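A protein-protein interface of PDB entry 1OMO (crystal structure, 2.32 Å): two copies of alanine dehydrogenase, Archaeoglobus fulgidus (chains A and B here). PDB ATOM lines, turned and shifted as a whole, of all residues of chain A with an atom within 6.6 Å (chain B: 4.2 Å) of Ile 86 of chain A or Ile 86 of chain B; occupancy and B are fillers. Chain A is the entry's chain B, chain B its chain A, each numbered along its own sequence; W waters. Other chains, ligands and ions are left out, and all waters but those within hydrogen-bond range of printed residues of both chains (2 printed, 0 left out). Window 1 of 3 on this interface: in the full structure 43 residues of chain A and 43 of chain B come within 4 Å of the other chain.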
ATOM      1  N   THR A   3     -10.511  20.554  38.314  1.00  0.00           N
ATOM      2  CA  THR A   3     -10.878  20.567  36.911  1.00  0.00           C
ATOM      3  C   THR A   3     -12.239  21.277  36.787  1.00  0.00           C
ATOM      4  O   THR A   3     -13.194  20.933  37.497  1.00  0.00           O
ATOM      5  CB  THR A   3     -10.990  19.109  36.402  1.00  0.00           C
ATOM      6  OG1 THR A   3      -9.695  18.493  36.474  1.00  0.00           O
ATOM      7  CG2 THR A   3     -11.524  19.056  34.945  1.00  0.00           C
ATOM      8  N   ALA A  62      -3.682  22.162  24.916  1.00  0.00           N
ATOM      9  CA  ALA A  62      -3.800  20.872  24.264  1.00  0.00           C
ATOM     10  C   ALA A  62      -5.180  20.387  24.706  1.00  0.00           C
ATOM     11  O   ALA A  62      -5.694  20.782  25.776  1.00  0.00           O
ATOM     12  CB  ALA A  62      -2.728  19.910  24.730  1.00  0.00           C
ATOM     13  N   GLY A  63      -5.785  19.550  23.881  1.00  0.00           N
ATOM     14  CA  GLY A  63      -7.092  19.046  24.224  1.00  0.00           C
ATOM     15  C   GLY A  63      -7.503  17.924  23.316  1.00  0.00           C
ATOM     16  O   GLY A  63      -6.944  17.751  22.232  1.00  0.00           O
ATOM     17  N   LEU A  64      -8.454  17.134  23.791  1.00  0.00           N
ATOM     18  CA  LEU A  64      -8.993  16.035  23.022  1.00  0.00           C
ATOM     19  C   LEU A  64     -10.513  16.122  23.042  1.00  0.00           C
ATOM     20  O   LEU A  64     -11.129  16.210  24.105  1.00  0.00           O
ATOM     21  CB  LEU A  64      -8.564  14.679  23.577  1.00  0.00           C
ATOM     22  CG  LEU A  64      -9.255  13.652  22.650  1.00  0.00           C
ATOM     23  CD1 LEU A  64      -8.256  12.631  22.156  1.00  0.00           C
ATOM     24  CD2 LEU A  64     -10.383  12.977  23.380  1.00  0.00           C
ATOM     25  N   LYS A  65     -11.114  16.145  21.861  1.00  0.00           N
ATOM     26  CA  LYS A  65     -12.553  16.174  21.776  1.00  0.00           C
ATOM     27  C   LYS A  65     -12.894  14.729  21.448  1.00  0.00           C
ATOM     28  O   LYS A  65     -12.268  14.141  20.572  1.00  0.00           O
ATOM     29  CB  LYS A  65     -13.025  17.082  20.643  1.00  0.00           C
ATOM     30  CG  LYS A  65     -14.546  17.127  20.542  1.00  0.00           C
ATOM     31  CD  LYS A  65     -15.007  18.091  19.517  1.00  0.00           C
ATOM     32  CE  LYS A  65     -15.159  17.407  18.198  1.00  0.00           C
ATOM     33  NZ  LYS A  65     -15.579  18.380  17.179  1.00  0.00           N
ATOM     34  N   TRP A  66     -13.848  14.161  22.179  1.00  0.00           N
ATOM     35  CA  TRP A  66     -14.304  12.784  21.996  1.00  0.00           C
ATOM     36  C   TRP A  66     -15.767  12.963  21.581  1.00  0.00           C
ATOM     37  O   TRP A  66     -16.609  13.386  22.396  1.00  0.00           O
ATOM     38  CB  TRP A  66     -14.181  12.071  23.340  1.00  0.00           C
ATOM     39  CG  TRP A  66     -14.593  10.635  23.376  1.00  0.00           C
ATOM     40  CD1 TRP A  66     -15.391  10.034  24.325  1.00  0.00           C
ATOM     41  CD2 TRP A  66     -14.092   9.572  22.545  1.00  0.00           C
ATOM     42  NE1 TRP A  66     -15.392   8.667  24.139  1.00  0.00           N
ATOM     43  CE2 TRP A  66     -14.601   8.356  23.062  1.00  0.00           C
ATOM     44  CE3 TRP A  66     -13.250   9.531  21.429  1.00  0.00           C
ATOM     45  CZ2 TRP A  66     -14.303   7.103  22.492  1.00  0.00           C
ATOM     46  CZ3 TRP A  66     -12.950   8.290  20.851  1.00  0.00           C
ATOM     47  CH2 TRP A  66     -13.475   7.082  21.392  1.00  0.00           C
ATOM     48  N   LEU A  84     -17.653  15.790  24.104  1.00  0.00           N
ATOM     49  CA  LEU A  84     -16.952  16.324  25.263  1.00  0.00           C
ATOM     50  C   LEU A  84     -15.529  16.658  24.863  1.00  0.00           C
ATOM     51  O   LEU A  84     -14.896  15.937  24.086  1.00  0.00           O
ATOM     52  CB  LEU A  84     -16.889  15.326  26.414  1.00  0.00           C
ATOM     53  CG  LEU A  84     -18.228  14.986  27.059  1.00  0.00           C
ATOM     54  CD1 LEU A  84     -18.006  13.987  28.229  1.00  0.00           C
ATOM     55  CD2 LEU A  84     -18.877  16.308  27.514  1.00  0.00           C
ATOM     56  N   MET A  85     -15.040  17.764  25.406  1.00  0.00           N
ATOM     57  CA  MET A  85     -13.685  18.215  25.169  1.00  0.00           C
ATOM     58  C   MET A  85     -13.007  18.254  26.532  1.00  0.00           C
ATOM     59  O   MET A  85     -13.580  18.778  27.484  1.00  0.00           O
ATOM     60  CB  MET A  85     -13.702  19.631  24.575  1.00  0.00           C
ATOM     61  CG  MET A  85     -12.402  20.438  24.742  1.00  0.00           C
ATOM     62  SD  MET A  85     -11.056  19.706  23.773  1.00  0.00           S
ATOM     63  CE  MET A  85     -11.488  20.306  22.057  1.00  0.00           C
ATOM     64  N   ILE A  86     -11.829  17.644  26.630  1.00  0.00           N
ATOM     65  CA  ILE A  86     -11.018  17.673  27.850  1.00  0.00           C
ATOM     66  C   ILE A  86      -9.949  18.641  27.385  1.00  0.00           C
ATOM     67  O   ILE A  86      -9.300  18.389  26.363  1.00  0.00           O
ATOM     68  CB  ILE A  86     -10.335  16.298  28.174  1.00  0.00           C
ATOM     69  CG1 ILE A  86     -11.398  15.219  28.430  1.00  0.00           C
ATOM     70  CG2 ILE A  86      -9.510  16.391  29.457  1.00  0.00           C
ATOM     71  CD1 ILE A  86     -10.861  13.783  28.613  1.00  0.00           C
ATOM     72  N   LEU A  87      -9.787  19.752  28.095  1.00  0.00           N
ATOM     73  CA  LEU A  87      -8.791  20.765  27.748  1.00  0.00           C
ATOM     74  C   LEU A  87      -7.636  20.663  28.774  1.00  0.00           C
ATOM     75  O   LEU A  87      -7.884  20.541  29.968  1.00  0.00           O
ATOM     76  CB  LEU A  87      -9.424  22.150  27.809  1.00  0.00           C
ATOM     77  CG  LEU A  87      -8.517  23.294  27.375  1.00  0.00           C
ATOM     78  CD1 LEU A  87      -8.324  23.198  25.870  1.00  0.00           C
ATOM     79  CD2 LEU A  87      -9.149  24.662  27.774  1.00  0.00           C
ATOM     80  N   ASN A  88      -6.389  20.726  28.311  1.00  0.00           N
ATOM     81  CA  ASN A  88      -5.246  20.535  29.202  1.00  0.00           C
ATOM     82  C   ASN A  88      -4.101  21.545  29.065  1.00  0.00           C
ATOM     83  O   ASN A  88      -3.926  22.188  28.021  1.00  0.00           O
ATOM     84  CB  ASN A  88      -4.615  19.159  28.953  1.00  0.00           C
ATOM     85  CG  ASN A  88      -5.617  18.016  28.976  1.00  0.00           C
ATOM     86  OD1 ASN A  88      -6.510  17.934  28.125  1.00  0.00           O
ATOM     87  ND2 ASN A  88      -5.461  17.111  29.936  1.00  0.00           N
ATOM     88  N   PRO A  95      -5.651  18.370  33.369  1.00  0.00           N
ATOM     89  CA  PRO A  95      -6.911  18.601  32.628  1.00  0.00           C
ATOM     90  C   PRO A  95      -7.641  19.775  33.300  1.00  0.00           C
ATOM     91  O   PRO A  95      -8.290  19.634  34.337  1.00  0.00           O
ATOM     92  CB  PRO A  95      -7.644  17.267  32.758  1.00  0.00           C
ATOM     93  CG  PRO A  95      -7.208  16.762  34.106  1.00  0.00           C
ATOM     94  CD  PRO A  95      -5.719  17.120  34.163  1.00  0.00           C
ATOM     95  N   LEU A  96      -7.470  20.944  32.704  1.00  0.00           N
ATOM     96  CA  LEU A  96      -8.033  22.171  33.213  1.00  0.00           C
ATOM     97  C   LEU A  96      -9.554  22.182  33.183  1.00  0.00           C
ATOM     98  O   LEU A  96     -10.179  22.740  34.094  1.00  0.00           O
ATOM     99  CB  LEU A  96      -7.503  23.328  32.389  1.00  0.00           C
ATOM    100  CG  LEU A  96      -5.977  23.452  32.358  1.00  0.00           C
ATOM    101  CD1 LEU A  96      -5.583  24.260  31.107  1.00  0.00           C
ATOM    102  CD2 LEU A  96      -5.488  24.140  33.636  1.00  0.00           C
ATOM    103  N   ALA A  97     -10.149  21.565  32.153  1.00  0.00           N
ATOM    104  CA  ALA A  97     -11.595  21.567  32.042  1.00  0.00           C
ATOM    105  C   ALA A  97     -12.125  20.406  31.201  1.00  0.00           C
ATOM    106  O   ALA A  97     -11.447  19.905  30.318  1.00  0.00           O
ATOM    107  CB  ALA A  97     -12.054  22.916  31.423  1.00  0.00           C
ATOM    108  N   VAL A  98     -13.327  19.964  31.520  1.00  0.00           N
ATOM    109  CA  VAL A  98     -14.017  18.932  30.750  1.00  0.00           C
ATOM    110  C   VAL A  98     -15.287  19.711  30.395  1.00  0.00           C
ATOM    111  O   VAL A  98     -16.056  20.088  31.274  1.00  0.00           O
ATOM    112  CB  VAL A  98     -14.369  17.700  31.594  1.00  0.00           C
ATOM    113  CG1 VAL A  98     -15.108  16.687  30.746  1.00  0.00           C
ATOM    114  CG2 VAL A  98     -13.099  17.051  32.114  1.00  0.00           C
ATOM    115  N   MET A  99     -15.496  19.990  29.121  1.00  0.00           N
ATOM    116  CA  MET A  99     -16.667  20.785  28.744  1.00  0.00           C
ATOM    117  C   MET A  99     -17.407  20.251  27.540  1.00  0.00           C
ATOM    118  O   MET A  99     -16.861  19.509  26.698  1.00  0.00           O
ATOM    119  CB  MET A  99     -16.242  22.211  28.414  1.00  0.00           C
ATOM    120  CG  MET A  99     -15.226  22.224  27.295  1.00  0.00           C
ATOM    121  SD  MET A  99     -14.693  23.832  26.681  1.00  0.00           S
ATOM    122  CE  MET A  99     -13.349  24.115  27.753  1.00  0.00           C
ATOM    123  N   VAL A 298      -9.956  22.927  19.735  1.00  0.00           N
ATOM    124  CA  VAL A 298      -9.122  23.358  20.840  1.00  0.00           C
ATOM    125  C   VAL A 298      -9.055  24.867  20.881  1.00  0.00           C
ATOM    126  O   VAL A 298      -9.129  25.459  21.953  1.00  0.00           O
ATOM    127  CB  VAL A 298      -7.696  22.757  20.759  1.00  0.00           C
ATOM    128  CG1 VAL A 298      -6.829  23.361  21.859  1.00  0.00           C
ATOM    129  CG2 VAL A 298      -7.763  21.227  20.952  1.00  0.00           C
ATOM    130  N   GLY B  63     -14.858   3.605  25.217  1.00  0.00           N
ATOM    131  CA  GLY B  63     -14.320   4.684  26.045  1.00  0.00           C
ATOM    132  C   GLY B  63     -12.999   5.195  25.539  1.00  0.00           C
ATOM    133  O   GLY B  63     -12.368   4.583  24.672  1.00  0.00           O
ATOM    134  N   LEU B  64     -12.569   6.332  26.061  1.00  0.00           N
ATOM    135  CA  LEU B  64     -11.281   6.882  25.665  1.00  0.00           C
ATOM    136  C   LEU B  64     -10.514   7.354  26.886  1.00  0.00           C
ATOM    137  O   LEU B  64     -11.044   8.130  27.665  1.00  0.00           O
ATOM    138  CB  LEU B  64     -11.449   8.061  24.690  1.00  0.00           C
ATOM    139  CG  LEU B  64     -10.047   8.624  24.333  1.00  0.00           C
ATOM    140  CD1 LEU B  64      -9.978   8.964  22.879  1.00  0.00           C
ATOM    141  CD2 LEU B  64      -9.717   9.855  25.177  1.00  0.00           C
ATOM    142  N   TRP B  66      -7.378   9.509  28.334  1.00  0.00           N
ATOM    143  CA  TRP B  66      -6.503  10.619  27.935  1.00  0.00           C
ATOM    144  C   TRP B  66      -5.544  10.840  29.127  1.00  0.00           C
ATOM    145  O   TRP B  66      -5.930  11.386  30.153  1.00  0.00           O
ATOM    146  CB  TRP B  66      -7.386  11.831  27.645  1.00  0.00           C
ATOM    147  CG  TRP B  66      -6.738  13.072  27.152  1.00  0.00           C
ATOM    148  CD1 TRP B  66      -6.932  14.319  27.654  1.00  0.00           C
ATOM    149  CD2 TRP B  66      -5.921  13.233  25.986  1.00  0.00           C
ATOM    150  NE1 TRP B  66      -6.302  15.252  26.878  1.00  0.00           N
ATOM    151  CE2 TRP B  66      -5.664  14.614  25.843  1.00  0.00           C
ATOM    152  CE3 TRP B  66      -5.370  12.342  25.049  1.00  0.00           C
ATOM    153  CZ2 TRP B  66      -4.884  15.142  24.785  1.00  0.00           C
ATOM    154  CZ3 TRP B  66      -4.592  12.855  23.997  1.00  0.00           C
ATOM    155  CH2 TRP B  66      -4.356  14.248  23.882  1.00  0.00           C
ATOM    156  N   LEU B  84      -7.801  10.498  32.714  1.00  0.00           N
ATOM    157  CA  LEU B  84      -9.244  10.617  32.715  1.00  0.00           C
ATOM    158  C   LEU B  84      -9.783   9.693  31.653  1.00  0.00           C
ATOM    159  O   LEU B  84      -9.251   9.649  30.532  1.00  0.00           O
ATOM    160  CB  LEU B  84      -9.684  12.026  32.369  1.00  0.00           C
ATOM    161  CG  LEU B  84      -9.538  13.102  33.424  1.00  0.00           C
ATOM    162  CD1 LEU B  84     -10.132  14.430  32.871  1.00  0.00           C
ATOM    163  CD2 LEU B  84     -10.228  12.645  34.711  1.00  0.00           C
ATOM    164  N   MET B  85     -10.851   8.983  32.012  1.00  0.00           N
ATOM    165  CA  MET B  85     -11.536   8.051  31.129  1.00  0.00           C
ATOM    166  C   MET B  85     -12.970   8.528  30.915  1.00  0.00           C
ATOM    167  O   MET B  85     -13.691   8.860  31.879  1.00  0.00           O
ATOM    168  CB  MET B  85     -11.570   6.651  31.769  1.00  0.00           C
ATOM    169  CG  MET B  85     -12.639   5.659  31.203  1.00  0.00           C
ATOM    170  SD  MET B  85     -12.364   5.247  29.457  1.00  0.00           S
ATOM    171  CE  MET B  85     -11.049   3.969  29.666  1.00  0.00           C
ATOM    172  N   ILE B  86     -13.362   8.587  29.648  1.00  0.00           N
ATOM    173  CA  ILE B  86     -14.724   8.929  29.284  1.00  0.00           C
ATOM    174  C   ILE B  86     -15.287   7.563  28.836  1.00  0.00           C
ATOM    175  O   ILE B  86     -14.756   6.931  27.913  1.00  0.00           O
ATOM    176  CB  ILE B  86     -14.821   9.942  28.109  1.00  0.00           C
ATOM    177  CG1 ILE B  86     -14.160  11.287  28.473  1.00  0.00           C
ATOM    178  CG2 ILE B  86     -16.311  10.157  27.790  1.00  0.00           C
ATOM    179  CD1 ILE B  86     -13.944  12.268  27.309  1.00  0.00           C
ATOM    180  N   LEU B  87     -16.332   7.097  29.516  1.00  0.00           N
ATOM    181  CA  LEU B  87     -16.964   5.804  29.228  1.00  0.00           C
ATOM    182  C   LEU B  87     -18.221   6.088  28.455  1.00  0.00           C
ATOM    183  O   LEU B  87     -19.047   6.861  28.925  1.00  0.00           O
ATOM    184  CB  LEU B  87     -17.383   5.095  30.518  1.00  0.00           C
ATOM    185  CG  LEU B  87     -17.009   3.661  30.860  1.00  0.00           C
ATOM    186  CD1 LEU B  87     -18.055   3.165  31.826  1.00  0.00           C
ATOM    187  CD2 LEU B  87     -16.957   2.761  29.676  1.00  0.00           C
ATOM    188  N   ASN B  88     -18.390   5.443  27.302  1.00  0.00           N
ATOM    189  CA  ASN B  88     -19.586   5.686  26.483  1.00  0.00           C
ATOM    190  C   ASN B  88     -20.405   4.440  26.195  1.00  0.00           C
ATOM    191  O   ASN B  88     -19.964   3.315  26.414  1.00  0.00           O
ATOM    192  CB  ASN B  88     -19.213   6.301  25.134  1.00  0.00           C
ATOM    193  CG  ASN B  88     -18.339   7.553  25.263  1.00  0.00           C
ATOM    194  OD1 ASN B  88     -17.214   7.501  25.789  1.00  0.00           O
ATOM    195  ND2 ASN B  88     -18.851   8.683  24.777  1.00  0.00           N
ATOM    196  N   PRO B  95     -21.985   9.650  26.682  1.00  0.00           N
ATOM    197  CA  PRO B  95     -20.911   9.627  27.687  1.00  0.00           C
ATOM    198  C   PRO B  95     -21.508   9.326  29.063  1.00  0.00           C
ATOM    199  O   PRO B  95     -21.939  10.238  29.789  1.00  0.00           O
ATOM    200  CB  PRO B  95     -20.316  11.035  27.608  1.00  0.00           C
ATOM    201  CG  PRO B  95     -21.496  11.876  27.223  1.00  0.00           C
ATOM    202  CD  PRO B  95     -22.233  11.018  26.190  1.00  0.00           C
ATOM    203  N   ALA B  97     -19.974   8.140  31.718  1.00  0.00           N
ATOM    204  CA  ALA B  97     -19.188   8.572  32.873  1.00  0.00           C
ATOM    205  C   ALA B  97     -17.847   9.198  32.481  1.00  0.00           C
ATOM    206  O   ALA B  97     -17.307   8.938  31.390  1.00  0.00           O
ATOM    207  CB  ALA B  97     -18.934   7.354  33.804  1.00  0.00           C
HETATM  208  O   HOH W   1     -18.316  11.714  24.253  1.00  0.00           O
HETATM  209  O   HOH W   2      -6.115  14.278  30.867  1.00  0.00           O
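The side-chain amide oxygen (OD1) of Asn 88 of chain A is in hydrogen-bond range of the indole nitrogen (NE1) of Trp 66 of chain B, at 3.0 Å. The indole nitrogen of Trp 66 of chain A sits at hydrogen-bond distance from the side-chain amide oxygen of Asn 88 of chain B (2.7 Å).
N of Leu 64 of chain A sits at hydrogen-bond distance from SD of Met 85 of chain A (3.7 Å). The side-chain sulfur of Met 85 of chain B lies within hydrogen-bond range of the backbone NH of Leu 64 of chain B (3.6 Å). O of Leu 84 of chain A is in hydrogen-bond range of N of Trp 66 of chain A (2.8 Å). The backbone carbonyl oxygen (O) of Ile 86 of chain B sits close to the side-chain amide oxygen (OD1) of Asn 88 of chain B (3.3 Å). O of Ala 62 of chain A is in hydrogen-bond range of N of Asn 88 of chain A. The backbone NH of Leu 64 of chain B is in hydrogen-bond range of the backbone carbonyl oxygen of Ile 86 of chain B, 2.9 Å away.
Among the printed residues, merely in contact across the chains: Trp 66 of chain A with Leu 64 of chain B (3.6 Å), Trp 66 of chain A with Ile 86 of chain B (3.6 Å), Leu 64 of chain A with Leu 64 of chain B (3.7 Å), Ile 86 of chain A with Ile 86 of chain B (3.7 Å), Leu 64 of chain A with Trp 66 of chain B (3.7 Å), Ile 86 of chain A with Trp 66 of chain B (3.8 Å), Pro 95 of chain A with Leu 84 of chain B (3.8 Å), Leu 84 of chain A with Pro 95 of chain B (3.8 Å), Trp 66 of chain A with Gly 63 of chain B (3.8 Å) and Ile 86 of chain A with Leu 84 of chain B (3.99 Å).
Of the printed residues of chain B, Ile 86 of chain A touches Trp 66, Leu 84 and Ile 86. Of the printed residues of chain B, Pro 95 of chain A touches Leu 84 (3.8 Å). Printed residues of chain A within 4 Å of Gly 63 of chain B: Trp 66 (3.8 Å). Of the printed residues of chain A, Leu 64 of chain B touches Leu 64 (3.7 Å) and Trp 66 (3.6 Å). Met 85 of chain B touches none of the printed residues of chain A. Ile 86 of chain B touches just these residues of chain A: Trp 66 (3.6 Å) and Ile 86 (3.7 Å). Of the printed residues of chain A, Pro 95 of chain B touches Leu 84 (3.8 Å). The nearest residue of chain A that does not touch Ile 86 of chain B is Leu 84 of chain A (4.2 Å). The nearest printed residue of chain B that does not touch Leu 84 of chain A is Ile 86 of chain B (4.2 Å).
Hydrophobic or aromatic side chains of chain A within 4 Å of the printed part of chain B: Leu 64, Trp 66, Leu 84, Ile 86 and Pro 95. Among the printed residues, 12 pairs touch across the chains.
Leu 64 of chain A touches Trp 66 of chain B, and with the chains exchanged Trp 66 of chain A touches Leu 64 of chain B. Leu 84 of chain A touches Pro 95 of chain B, and with the chains exchanged Pro 95 of chain A touches Leu 84 of chain B. Ile 86 of chain A touches Leu 84 of chain B, but with the chains exchanged Leu 84 of chain A does not touch Ile 86 of chain B (4.2 Å). Ile 86 of chain A touches its own counterpart, Ile 86 of chain B. Of the 12 pairs that touch across the chains among the printed residues, 10 have their exchanged pair printed and touching as well.
Water W2 bridges the backbone carbonyl oxygen of Trp 66 of chain B (3.0 Å) and the side-chain amide nitrogen of Asn 88 of chain A (3.1 Å). Water W1 lies within hydrogen-bond range of O of Trp 66 of chain A (3.0 Å) and ND2 of Asn 88 of chain B (3.1 Å).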
